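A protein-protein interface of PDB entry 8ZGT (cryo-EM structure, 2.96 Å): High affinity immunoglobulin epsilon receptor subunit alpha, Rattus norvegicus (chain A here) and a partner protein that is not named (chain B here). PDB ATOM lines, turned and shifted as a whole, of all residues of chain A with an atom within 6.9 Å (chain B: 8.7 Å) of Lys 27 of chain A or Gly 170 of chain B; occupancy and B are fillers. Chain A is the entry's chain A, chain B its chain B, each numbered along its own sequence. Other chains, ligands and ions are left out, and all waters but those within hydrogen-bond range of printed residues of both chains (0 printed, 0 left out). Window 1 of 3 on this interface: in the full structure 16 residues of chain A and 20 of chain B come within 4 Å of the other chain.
The side-chain amino group of Lys 27 of chain A sits at hydrogen-bond distance from the side-chain hydroxyl of Tyr 158 of chain B.
The side-chain amino group (NZ) of Lys 27 of chain A lies within salt-bridge range of the side-chain carboxylate (OD1) of Asp 168 of chain B, 2.9 Å away.
The side-chain amino group (NZ) of Lys 98 of chain A is in hydrogen-bond range of the backbone carbonyl oxygen (O) of Phe 88 of chain B, at 3.3 Å.
The side-chain carboxylate of Asp 89 of chain B is in hydrogen-bond range of the backbone NH of Lys 98 of chain A.
The side-chain amide oxygen (OD1) of Asn 50 of chain A lies within hydrogen-bond range of the side-chain amide nitrogen (NE2) of Gln 26 of chain A (3.0 Å).
The backbone NH (N) of Tyr 97 of chain A lies within hydrogen-bond range of the backbone carbonyl oxygen (O) of Gln 26 of chain A.
OG of Ser 28 of chain A sits at hydrogen-bond distance from O of Tyr 97 of chain A (2.8 Å).
SG of Cys 162 of chain B is disulfide-bonded to SG of Cys 171 of chain B, at 2.0 Å.
Among the printed residues, pairs that only touch across the chains: Thr 25 of chain A with Tyr 161 of chain B, Tyr 97 of chain A with Asp 89 of chain B, Gln 26 of chain A with Tyr 161 of chain B, Lys 100 of chain A with Asp 168 of chain B, Lys 27 of chain A with Gly 170 of chain B, Lys 98 of chain A with Asp 87 of chain B and Tyr 97 of chain A with Tyr 158 of chain B.
Lys 27 of chain A touches just these residues of chain B: Tyr 158 (3.4 Å), Asp 168 (2.9 Å) and Gly 170 (3.97 Å).
No residue of chain B comes within 4 Å of Ser 28 of chain A.
Of the printed residues of chain A, Phe 88 of chain B touches Lys 98.
Printed residues of chain A within 4 Å of Asp 89 of chain B: Tyr 97 (3.4 Å) and Lys 98 (3.3 Å).
Printed residues of chain B within 4 Å of Tyr 97 of chain A: Asp 89 (3.4 Å) and Tyr 158 (3.98 Å).
Cys 162 of chain B touches none of the printed residues of chain A.
Among the printed residues, Asp or Glu carboxylates within 4 Å of a Lys or Arg side-chain nitrogen of the other chain: Lys 27 of chain A with Asp 168 of chain B.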
ATOM      1  N   THR A  25      36.380   8.161 -22.391  1.00  0.00           N
ATOM      2  CA  THR A  25      35.807   6.950 -21.818  1.00  0.00           C
ATOM      3  C   THR A  25      34.280   7.061 -21.688  1.00  0.00           C
ATOM      4  O   THR A  25      33.558   6.689 -22.612  1.00  0.00           O
ATOM      5  CB  THR A  25      36.459   6.619 -20.448  1.00  0.00           C
ATOM      6  OG1 THR A  25      35.762   7.280 -19.392  1.00  0.00           O
ATOM      7  CG2 THR A  25      37.916   7.051 -20.422  1.00  0.00           C
ATOM      8  N   GLN A  26      33.783   7.579 -20.566  1.00  0.00           N
ATOM      9  CA  GLN A  26      32.345   7.623 -20.328  1.00  0.00           C
ATOM     10  C   GLN A  26      31.754   8.868 -20.993  1.00  0.00           C
ATOM     11  O   GLN A  26      32.428   9.578 -21.744  1.00  0.00           O
ATOM     12  CB  GLN A  26      32.044   7.547 -18.826  1.00  0.00           C
ATOM     13  CG  GLN A  26      32.224   8.829 -17.981  1.00  0.00           C
ATOM     14  CD  GLN A  26      33.632   9.388 -17.958  1.00  0.00           C
ATOM     15  OE1 GLN A  26      34.608   8.650 -18.029  1.00  0.00           O
ATOM     16  NE2 GLN A  26      33.739  10.706 -17.852  1.00  0.00           N
ATOM     17  N   LYS A  27      30.469   9.124 -20.759  1.00  0.00           N
ATOM     18  CA  LYS A  27      29.862  10.366 -21.213  1.00  0.00           C
ATOM     19  C   LYS A  27      30.424  11.552 -20.436  1.00  0.00           C
ATOM     20  O   LYS A  27      30.704  11.464 -19.239  1.00  0.00           O
ATOM     21  CB  LYS A  27      28.345  10.318 -21.044  1.00  0.00           C
ATOM     22  CG  LYS A  27      27.659   9.180 -21.776  1.00  0.00           C
ATOM     23  CD  LYS A  27      26.160   9.153 -21.497  1.00  0.00           C
ATOM     24  CE  LYS A  27      25.517  10.502 -21.794  1.00  0.00           C
ATOM     25  NZ  LYS A  27      24.089  10.372 -22.192  1.00  0.00           N
ATOM     26  N   SER A  28      30.587  12.670 -21.134  1.00  0.00           N
ATOM     27  CA  SER A  28      31.058  13.887 -20.495  1.00  0.00           C
ATOM     28  C   SER A  28      29.966  14.484 -19.611  1.00  0.00           C
ATOM     29  O   SER A  28      28.777  14.191 -19.760  1.00  0.00           O
ATOM     30  CB  SER A  28      31.505  14.902 -21.543  1.00  0.00           C
ATOM     31  OG  SER A  28      32.386  14.307 -22.476  1.00  0.00           O
ATOM     32  N   VAL A  29      30.389  15.304 -18.652  1.00  0.00           N
ATOM     33  CA  VAL A  29      29.482  16.006 -17.751  1.00  0.00           C
ATOM     34  C   VAL A  29      29.791  17.492 -17.835  1.00  0.00           C
ATOM     35  O   VAL A  29      30.936  17.901 -17.623  1.00  0.00           O
ATOM     36  CB  VAL A  29      29.609  15.511 -16.296  1.00  0.00           C
ATOM     37  CG1 VAL A  29      28.672  16.286 -15.389  1.00  0.00           C
ATOM     38  CG2 VAL A  29      29.323  14.021 -16.198  1.00  0.00           C
ATOM     39  N   ASN A  50      34.143  17.906 -18.446  1.00  0.00           N
ATOM     40  CA  ASN A  50      34.162  16.701 -17.601  1.00  0.00           C
ATOM     41  C   ASN A  50      34.645  16.891 -16.159  1.00  0.00           C
ATOM     42  O   ASN A  50      34.241  16.138 -15.267  1.00  0.00           O
ATOM     43  CB  ASN A  50      35.035  15.636 -18.279  1.00  0.00           C
ATOM     44  CG  ASN A  50      34.679  14.211 -17.864  1.00  0.00           C
ATOM     45  OD1 ASN A  50      35.297  13.256 -18.332  1.00  0.00           O
ATOM     46  ND2 ASN A  50      33.659  14.058 -17.026  1.00  0.00           N
ATOM     47  N   CYS A  91      28.998  19.723 -23.998  1.00  0.00           N
ATOM     48  CA  CYS A  91      30.448  19.639 -24.104  1.00  0.00           C
ATOM     49  C   CYS A  91      30.867  18.211 -24.424  1.00  0.00           C
ATOM     50  O   CYS A  91      30.197  17.249 -24.041  1.00  0.00           O
ATOM     51  CB  CYS A  91      31.140  20.122 -22.819  1.00  0.00           C
ATOM     52  SG  CYS A  91      31.750  18.866 -21.646  1.00  0.00           S
ATOM     53  N   PHE A  96      35.860  11.032 -25.504  1.00  0.00           N
ATOM     54  CA  PHE A  96      34.660  10.854 -24.696  1.00  0.00           C
ATOM     55  C   PHE A  96      33.428  11.041 -25.577  1.00  0.00           C
ATOM     56  O   PHE A  96      33.522  11.437 -26.740  1.00  0.00           O
ATOM     57  CB  PHE A  96      34.641  11.839 -23.519  1.00  0.00           C
ATOM     58  CG  PHE A  96      35.643  11.530 -22.432  1.00  0.00           C
ATOM     59  CD1 PHE A  96      36.991  11.821 -22.598  1.00  0.00           C
ATOM     60  CD2 PHE A  96      35.228  10.980 -21.231  1.00  0.00           C
ATOM     61  CE1 PHE A  96      37.905  11.542 -21.599  1.00  0.00           C
ATOM     62  CE2 PHE A  96      36.136  10.698 -20.228  1.00  0.00           C
ATOM     63  CZ  PHE A  96      37.476  10.981 -20.413  1.00  0.00           C
ATOM     64  N   TYR A  97      32.259  10.752 -25.009  1.00  0.00           N
ATOM     65  CA  TYR A  97      31.000  10.949 -25.707  1.00  0.00           C
ATOM     66  C   TYR A  97      30.450  12.341 -25.405  1.00  0.00           C
ATOM     67  O   TYR A  97      31.018  13.107 -24.625  1.00  0.00           O
ATOM     68  CB  TYR A  97      29.994   9.869 -25.317  1.00  0.00           C
ATOM     69  CG  TYR A  97      30.487   8.459 -25.531  1.00  0.00           C
ATOM     70  CD1 TYR A  97      31.008   8.062 -26.755  1.00  0.00           C
ATOM     71  CD2 TYR A  97      30.428   7.523 -24.508  1.00  0.00           C
ATOM     72  CE1 TYR A  97      31.461   6.773 -26.953  1.00  0.00           C
ATOM     73  CE2 TYR A  97      30.879   6.232 -24.696  1.00  0.00           C
ATOM     74  CZ  TYR A  97      31.394   5.864 -25.920  1.00  0.00           C
ATOM     75  OH  TYR A  97      31.842   4.578 -26.111  1.00  0.00           O
ATOM     76  N   LYS A  98      29.330  12.677 -26.036  1.00  0.00           N
ATOM     77  CA  LYS A  98      28.680  13.949 -25.771  1.00  0.00           C
ATOM     78  C   LYS A  98      27.993  13.920 -24.409  1.00  0.00           C
ATOM     79  O   LYS A  98      27.717  12.861 -23.842  1.00  0.00           O
ATOM     80  CB  LYS A  98      27.671  14.279 -26.869  1.00  0.00           C
ATOM     81  CG  LYS A  98      28.309  14.757 -28.156  1.00  0.00           C
ATOM     82  CD  LYS A  98      27.287  15.337 -29.106  1.00  0.00           C
ATOM     83  CE  LYS A  98      27.908  15.608 -30.460  1.00  0.00           C
ATOM     84  NZ  LYS A  98      26.897  15.999 -31.472  1.00  0.00           N
ATOM     85  N   SER A  99      27.720  15.106 -23.887  1.00  0.00           N
ATOM     86  CA  SER A  99      27.198  15.260 -22.540  1.00  0.00           C
ATOM     87  C   SER A  99      25.678  15.366 -22.546  1.00  0.00           C
ATOM     88  O   SER A  99      25.044  15.610 -23.574  1.00  0.00           O
ATOM     89  CB  SER A  99      27.804  16.497 -21.876  1.00  0.00           C
ATOM     90  OG  SER A  99      27.137  17.667 -22.304  1.00  0.00           O
ATOM     91  N   LYS A 100      25.100  15.162 -21.372  1.00  0.00           N
ATOM     92  CA  LYS A 100      23.705  15.509 -21.154  1.00  0.00           C
ATOM     93  C   LYS A 100      23.573  17.028 -21.172  1.00  0.00           C
ATOM     94  O   LYS A 100      24.360  17.716 -20.515  1.00  0.00           O
ATOM     95  CB  LYS A 100      23.226  14.936 -19.822  1.00  0.00           C
ATOM     96  CG  LYS A 100      21.735  15.058 -19.573  1.00  0.00           C
ATOM     97  CD  LYS A 100      21.443  15.329 -18.108  1.00  0.00           C
ATOM     98  CE  LYS A 100      21.628  14.078 -17.270  1.00  0.00           C
ATOM     99  NZ  LYS A 100      20.403  13.233 -17.268  1.00  0.00           N
ATOM    100  N   ASP B  87      22.496  16.397 -30.727  1.00  0.00           N
ATOM    101  CA  ASP B  87      22.618  16.039 -29.322  1.00  0.00           C
ATOM    102  C   ASP B  87      23.229  14.663 -29.105  1.00  0.00           C
ATOM    103  O   ASP B  87      23.607  14.344 -27.973  1.00  0.00           O
ATOM    104  CB  ASP B  87      21.244  16.084 -28.646  1.00  0.00           C
ATOM    105  CG  ASP B  87      20.638  17.470 -28.647  1.00  0.00           C
ATOM    106  OD1 ASP B  87      21.254  18.392 -29.220  1.00  0.00           O
ATOM    107  OD2 ASP B  87      19.543  17.639 -28.073  1.00  0.00           O
ATOM    108  N   PHE B  88      23.339  13.848 -30.151  1.00  0.00           N
ATOM    109  CA  PHE B  88      23.803  12.476 -30.038  1.00  0.00           C
ATOM    110  C   PHE B  88      25.083  12.288 -30.841  1.00  0.00           C
ATOM    111  O   PHE B  88      25.388  13.056 -31.757  1.00  0.00           O
ATOM    112  CB  PHE B  88      22.727  11.492 -30.512  1.00  0.00           C
ATOM    113  CG  PHE B  88      21.358  11.801 -29.982  1.00  0.00           C
ATOM    114  CD1 PHE B  88      21.060  11.607 -28.642  1.00  0.00           C
ATOM    115  CD2 PHE B  88      20.372  12.297 -30.820  1.00  0.00           C
ATOM    116  CE1 PHE B  88      19.803  11.897 -28.147  1.00  0.00           C
ATOM    117  CE2 PHE B  88      19.112  12.588 -30.331  1.00  0.00           C
ATOM    118  CZ  PHE B  88      18.828  12.388 -28.994  1.00  0.00           C
ATOM    119  N   ASP B  89      25.829  11.248 -30.478  1.00  0.00           N
ATOM    120  CA  ASP B  89      27.143  11.005 -31.050  1.00  0.00           C
ATOM    121  C   ASP B  89      27.036  10.501 -32.485  1.00  0.00           C
ATOM    122  O   ASP B  89      26.019   9.947 -32.907  1.00  0.00           O
ATOM    123  CB  ASP B  89      27.911   9.992 -30.206  1.00  0.00           C
ATOM    124  CG  ASP B  89      28.390  10.573 -28.900  1.00  0.00           C
ATOM    125  OD1 ASP B  89      27.577  10.666 -27.957  1.00  0.00           O
ATOM    126  OD2 ASP B  89      29.580  10.937 -28.816  1.00  0.00           O
ATOM    127  N   VAL B  92      27.121   6.408 -32.703  1.00  0.00           N
ATOM    128  CA  VAL B  92      25.841   5.719 -32.573  1.00  0.00           C
ATOM    129  C   VAL B  92      25.051   5.804 -33.873  1.00  0.00           C
ATOM    130  O   VAL B  92      24.449   4.819 -34.318  1.00  0.00           O
ATOM    131  CB  VAL B  92      25.054   6.306 -31.389  1.00  0.00           C
ATOM    132  CG1 VAL B  92      23.715   5.612 -31.225  1.00  0.00           C
ATOM    133  CG2 VAL B  92      25.869   6.199 -30.121  1.00  0.00           C
ATOM    134  N   ASN B 155      27.180   0.535 -30.894  1.00  0.00           N
ATOM    135  CA  ASN B 155      26.065   0.546 -29.953  1.00  0.00           C
ATOM    136  C   ASN B 155      26.371  -0.285 -28.716  1.00  0.00           C
ATOM    137  O   ASN B 155      26.004   0.102 -27.603  1.00  0.00           O
ATOM    138  CB  ASN B 155      24.805   0.023 -30.634  1.00  0.00           C
ATOM    139  CG  ASN B 155      24.175   1.038 -31.547  1.00  0.00           C
ATOM    140  OD1 ASN B 155      24.552   2.208 -31.552  1.00  0.00           O
ATOM    141  ND2 ASN B 155      23.215   0.593 -32.342  1.00  0.00           N
ATOM    142  N   TYR B 158      28.807   1.701 -26.557  1.00  0.00           N
ATOM    143  CA  TYR B 158      28.129   2.741 -25.784  1.00  0.00           C
ATOM    144  C   TYR B 158      27.282   2.126 -24.672  1.00  0.00           C
ATOM    145  O   TYR B 158      27.311   2.605 -23.533  1.00  0.00           O
ATOM    146  CB  TYR B 158      27.294   3.627 -26.725  1.00  0.00           C
ATOM    147  CG  TYR B 158      26.769   4.965 -26.179  1.00  0.00           C
ATOM    148  CD1 TYR B 158      25.894   5.040 -25.091  1.00  0.00           C
ATOM    149  CD2 TYR B 158      27.179   6.159 -26.754  1.00  0.00           C
ATOM    150  CE1 TYR B 158      25.439   6.251 -24.616  1.00  0.00           C
ATOM    151  CE2 TYR B 158      26.727   7.377 -26.282  1.00  0.00           C
ATOM    152  CZ  TYR B 158      25.859   7.414 -25.214  1.00  0.00           C
ATOM    153  OH  TYR B 158      25.409   8.624 -24.741  1.00  0.00           O
ATOM    154  N   MET B 159      26.532   1.062 -24.973  1.00  0.00           N
ATOM    155  CA  MET B 159      25.606   0.470 -24.016  1.00  0.00           C
ATOM    156  C   MET B 159      26.301  -0.308 -22.909  1.00  0.00           C
ATOM    157  O   MET B 159      25.632  -0.720 -21.955  1.00  0.00           O
ATOM    158  CB  MET B 159      24.617  -0.448 -24.740  1.00  0.00           C
ATOM    159  CG  MET B 159      23.283   0.205 -25.066  1.00  0.00           C
ATOM    160  SD  MET B 159      22.791   1.440 -23.851  1.00  0.00           S
ATOM    161  CE  MET B 159      21.778   0.451 -22.754  1.00  0.00           C
ATOM    162  N   TYR B 161      28.408   1.342 -21.123  1.00  0.00           N
ATOM    163  CA  TYR B 161      28.464   2.443 -20.157  1.00  0.00           C
ATOM    164  C   TYR B 161      27.077   3.020 -19.881  1.00  0.00           C
ATOM    165  O   TYR B 161      26.872   4.232 -19.926  1.00  0.00           O
ATOM    166  CB  TYR B 161      29.416   3.528 -20.656  1.00  0.00           C
ATOM    167  CG  TYR B 161      30.904   3.194 -20.646  1.00  0.00           C
ATOM    168  CD1 TYR B 161      31.378   1.936 -20.272  1.00  0.00           C
ATOM    169  CD2 TYR B 161      31.835   4.138 -21.054  1.00  0.00           C
ATOM    170  CE1 TYR B 161      32.731   1.646 -20.280  1.00  0.00           C
ATOM    171  CE2 TYR B 161      33.188   3.857 -21.067  1.00  0.00           C
ATOM    172  CZ  TYR B 161      33.630   2.612 -20.681  1.00  0.00           C
ATOM    173  OH  TYR B 161      34.976   2.334 -20.695  1.00  0.00           O
ATOM    174  N   CYS B 162      26.110   2.156 -19.577  1.00  0.00           N
ATOM    175  CA  CYS B 162      24.760   2.575 -19.208  1.00  0.00           C
ATOM    176  C   CYS B 162      24.227   1.553 -18.218  1.00  0.00           C
ATOM    177  O   CYS B 162      24.108   0.373 -18.557  1.00  0.00           O
ATOM    178  CB  CYS B 162      23.829   2.669 -20.428  1.00  0.00           C
ATOM    179  SG  CYS B 162      24.024   4.112 -21.527  1.00  0.00           S
ATOM    180  N   ASP B 164      21.235   1.394 -17.035  1.00  0.00           N
ATOM    181  CA  ASP B 164      19.848   1.066 -17.318  1.00  0.00           C
ATOM    182  C   ASP B 164      19.496   1.578 -18.705  1.00  0.00           C
ATOM    183  O   ASP B 164      20.175   2.445 -19.260  1.00  0.00           O
ATOM    184  CB  ASP B 164      18.904   1.661 -16.264  1.00  0.00           C
ATOM    185  CG  ASP B 164      17.584   0.921 -16.178  1.00  0.00           C
ATOM    186  OD1 ASP B 164      17.514  -0.233 -16.651  1.00  0.00           O
ATOM    187  OD2 ASP B 164      16.613   1.494 -15.638  1.00  0.00           O
ATOM    188  N   ILE B 165      18.416   1.027 -19.263  1.00  0.00           N
ATOM    189  CA  ILE B 165      17.922   1.468 -20.566  1.00  0.00           C
ATOM    190  C   ILE B 165      17.206   2.807 -20.496  1.00  0.00           C
ATOM    191  O   ILE B 165      16.945   3.416 -21.541  1.00  0.00           O
ATOM    192  CB  ILE B 165      17.011   0.371 -21.158  1.00  0.00           C
ATOM    193  CG1 ILE B 165      17.076   0.366 -22.685  1.00  0.00           C
ATOM    194  CG2 ILE B 165      15.568   0.516 -20.672  1.00  0.00           C
ATOM    195  CD1 ILE B 165      16.223  -0.701 -23.328  1.00  0.00           C
ATOM    196  N   THR B 166      16.906   3.298 -19.295  1.00  0.00           N
ATOM    197  CA  THR B 166      16.120   4.510 -19.103  1.00  0.00           C
ATOM    198  C   THR B 166      16.872   5.513 -18.238  1.00  0.00           C
ATOM    199  O   THR B 166      16.274   6.244 -17.444  1.00  0.00           O
ATOM    200  CB  THR B 166      14.766   4.177 -18.484  1.00  0.00           C
ATOM    201  OG1 THR B 166      14.924   3.106 -17.545  1.00  0.00           O
ATOM    202  CG2 THR B 166      13.790   3.739 -19.559  1.00  0.00           C
ATOM    203  N   GLU B 167      18.202   5.547 -18.365  1.00  0.00           N
ATOM    204  CA  GLU B 167      19.002   6.515 -17.619  1.00  0.00           C
ATOM    205  C   GLU B 167      18.767   7.937 -18.117  1.00  0.00           C
ATOM    206  O   GLU B 167      18.474   8.841 -17.326  1.00  0.00           O
ATOM    207  CB  GLU B 167      20.483   6.165 -17.726  1.00  0.00           C
ATOM    208  CG  GLU B 167      21.027   5.287 -16.629  1.00  0.00           C
ATOM    209  CD  GLU B 167      22.495   5.559 -16.379  1.00  0.00           C
ATOM    210  OE1 GLU B 167      22.938   6.698 -16.634  1.00  0.00           O
ATOM    211  OE2 GLU B 167      23.207   4.640 -15.934  1.00  0.00           O
ATOM    212  N   ASP B 168      18.885   8.148 -19.423  1.00  0.00           N
ATOM    213  CA  ASP B 168      18.742   9.472 -20.020  1.00  0.00           C
ATOM    214  C   ASP B 168      18.360   9.293 -21.485  1.00  0.00           C
ATOM    215  O   ASP B 168      17.929   8.214 -21.907  1.00  0.00           O
ATOM    216  CB  ASP B 168      20.022  10.299 -19.865  1.00  0.00           C
ATOM    217  CG  ASP B 168      21.275   9.461 -19.982  1.00  0.00           C
ATOM    218  OD1 ASP B 168      22.382  10.032 -19.889  1.00  0.00           O
ATOM    219  OD2 ASP B 168      21.157   8.242 -20.202  1.00  0.00           O
ATOM    220  N   ASP B 169      18.520  10.366 -22.265  1.00  0.00           N
ATOM    221  CA  ASP B 169      18.167  10.305 -23.676  1.00  0.00           C
ATOM    222  C   ASP B 169      19.189   9.502 -24.467  1.00  0.00           C
ATOM    223  O   ASP B 169      18.841   8.906 -25.492  1.00  0.00           O
ATOM    224  CB  ASP B 169      18.069  11.711 -24.261  1.00  0.00           C
ATOM    225  CG  ASP B 169      16.863  12.472 -23.750  1.00  0.00           C
ATOM    226  OD1 ASP B 169      15.984  11.836 -23.140  1.00  0.00           O
ATOM    227  OD2 ASP B 169      16.775  13.697 -23.972  1.00  0.00           O
ATOM    228  N   GLY B 170      20.443   9.475 -24.004  1.00  0.00           N
ATOM    229  CA  GLY B 170      21.495   8.810 -24.759  1.00  0.00           C
ATOM    230  C   GLY B 170      21.333   7.303 -24.811  1.00  0.00           C
ATOM    231  O   GLY B 170      21.370   6.706 -25.890  1.00  0.00           O
ATOM    232  N   CYS B 171      21.123   6.671 -23.650  1.00  0.00           N
ATOM    233  CA  CYS B 171      20.972   5.218 -23.609  1.00  0.00           C
ATOM    234  C   CYS B 171      19.666   4.775 -24.259  1.00  0.00           C
ATOM    235  O   CYS B 171      19.623   3.735 -24.925  1.00  0.00           O
ATOM    236  CB  CYS B 171      21.057   4.707 -22.166  1.00  0.00           C
ATOM    237  SG  CYS B 171      22.437   5.335 -21.149  1.00  0.00           S
ATOM    238  N   PHE B 172      18.600   5.568 -24.106  1.00  0.00           N
ATOM    239  CA  PHE B 172      17.317   5.233 -24.721  1.00  0.00           C
ATOM    240  C   PHE B 172      17.377   5.344 -26.242  1.00  0.00           C
ATOM    241  O   PHE B 172      16.868   4.467 -26.954  1.00  0.00           O
ATOM    242  CB  PHE B 172      16.221   6.136 -24.160  1.00  0.00           C
ATOM    243  CG  PHE B 172      14.829   5.655 -24.452  1.00  0.00           C
ATOM    244  CD1 PHE B 172      14.253   4.655 -23.683  1.00  0.00           C
ATOM    245  CD2 PHE B 172      14.095   6.201 -25.495  1.00  0.00           C
ATOM    246  CE1 PHE B 172      12.973   4.209 -23.949  1.00  0.00           C
ATOM    247  CE2 PHE B 172      12.814   5.758 -25.766  1.00  0.00           C
ATOM    248  CZ  PHE B 172      12.254   4.762 -24.991  1.00  0.00           C
ATOM    249  N   VAL B 173      18.006   6.406 -26.755  1.00  0.00           N
ATOM    250  CA  VAL B 173      18.141   6.579 -28.199  1.00  0.00           C
ATOM    251  C   VAL B 173      19.083   5.527 -28.781  1.00  0.00           C
ATOM    252  O   VAL B 173      18.829   4.984 -29.864  1.00  0.00           O
ATOM    253  CB  VAL B 173      18.583   8.026 -28.508  1.00  0.00           C
ATOM    254  CG1 VAL B 173      19.302   8.149 -29.848  1.00  0.00           C
ATOM    255  CG2 VAL B 173      17.376   8.952 -28.486  1.00  0.00           C
ATOM    256  N   THR B 174      20.147   5.177 -28.046  1.00  0.00           N
ATOM    257  CA  THR B 174      21.047   4.111 -28.485  1.00  0.00           C
ATOM    258  C   THR B 174      20.348   2.755 -28.510  1.00  0.00           C
ATOM    259  O   THR B 174      20.577   1.955 -29.422  1.00  0.00           O
ATOM    260  CB  THR B 174      22.279   4.060 -27.584  1.00  0.00           C
ATOM    261  OG1 THR B 174      22.719   5.393 -27.300  1.00  0.00           O
ATOM    262  CG2 THR B 174      23.405   3.301 -28.261  1.00  0.00           C
ATOM    263  N   SER B 175      19.474   2.486 -27.534  1.00  0.00           N
ATOM    264  CA  SER B 175      18.729   1.230 -27.532  1.00  0.00           C
ATOM    265  C   SER B 175      17.723   1.166 -28.678  1.00  0.00           C
ATOM    266  O   SER B 175      17.584   0.120 -29.327  1.00  0.00           O
ATOM    267  CB  SER B 175      18.024   1.049 -26.191  1.00  0.00           C
ATOM    268  OG  SER B 175      16.779   1.720 -26.177  1.00  0.00           O
ATOM    269  N   PHE B 176      17.020   2.275 -28.943  1.00  0.00           N
ATOM    270  CA  PHE B 176      16.076   2.318 -30.061  1.00  0.00           C
ATOM    271  C   PHE B 176      16.792   2.162 -31.399  1.00  0.00           C
ATOM    272  O   PHE B 176      16.315   1.449 -32.296  1.00  0.00           O
ATOM    273  CB  PHE B 176      15.287   3.627 -30.010  1.00  0.00           C
ATOM    274  CG  PHE B 176      14.515   3.926 -31.263  1.00  0.00           C
ATOM    275  CD1 PHE B 176      13.392   3.183 -31.595  1.00  0.00           C
ATOM    276  CD2 PHE B 176      14.903   4.960 -32.103  1.00  0.00           C
ATOM    277  CE1 PHE B 176      12.679   3.459 -32.746  1.00  0.00           C
ATOM    278  CE2 PHE B 176      14.194   5.239 -33.256  1.00  0.00           C
ATOM    279  CZ  PHE B 176      13.081   4.488 -33.576  1.00  0.00           C
ATOM    280  N   ILE B 177      17.962   2.788 -31.535  1.00  0.00           N
ATOM    281  CA  ILE B 177      18.768   2.639 -32.738  1.00  0.00           C
ATOM    282  C   ILE B 177      19.326   1.218 -32.842  1.00  0.00           C
ATOM    283  O   ILE B 177      19.511   0.702 -33.946  1.00  0.00           O
ATOM    284  CB  ILE B 177      19.848   3.747 -32.756  1.00  0.00           C
ATOM    285  CG1 ILE B 177      19.503   4.811 -33.799  1.00  0.00           C
ATOM    286  CG2 ILE B 177      21.254   3.224 -33.001  1.00  0.00           C
ATOM    287  CD1 ILE B 177      18.294   5.640 -33.451  1.00  0.00           C
ATOM    288  N   THR B 178      19.541   0.541 -31.707  1.00  0.00           N
ATOM    289  CA  THR B 178      19.959  -0.861 -31.731  1.00  0.00           C
ATOM    290  C   THR B 178      18.859  -1.779 -32.265  1.00  0.00           C
ATOM    291  O   THR B 178      19.141  -2.688 -33.059  1.00  0.00           O
ATOM    292  CB  THR B 178      20.395  -1.299 -30.332  1.00  0.00           C
ATOM    293  OG1 THR B 178      21.344  -0.360 -29.812  1.00  0.00           O
ATOM    294  CG2 THR B 178      21.026  -2.679 -30.364  1.00  0.00           C
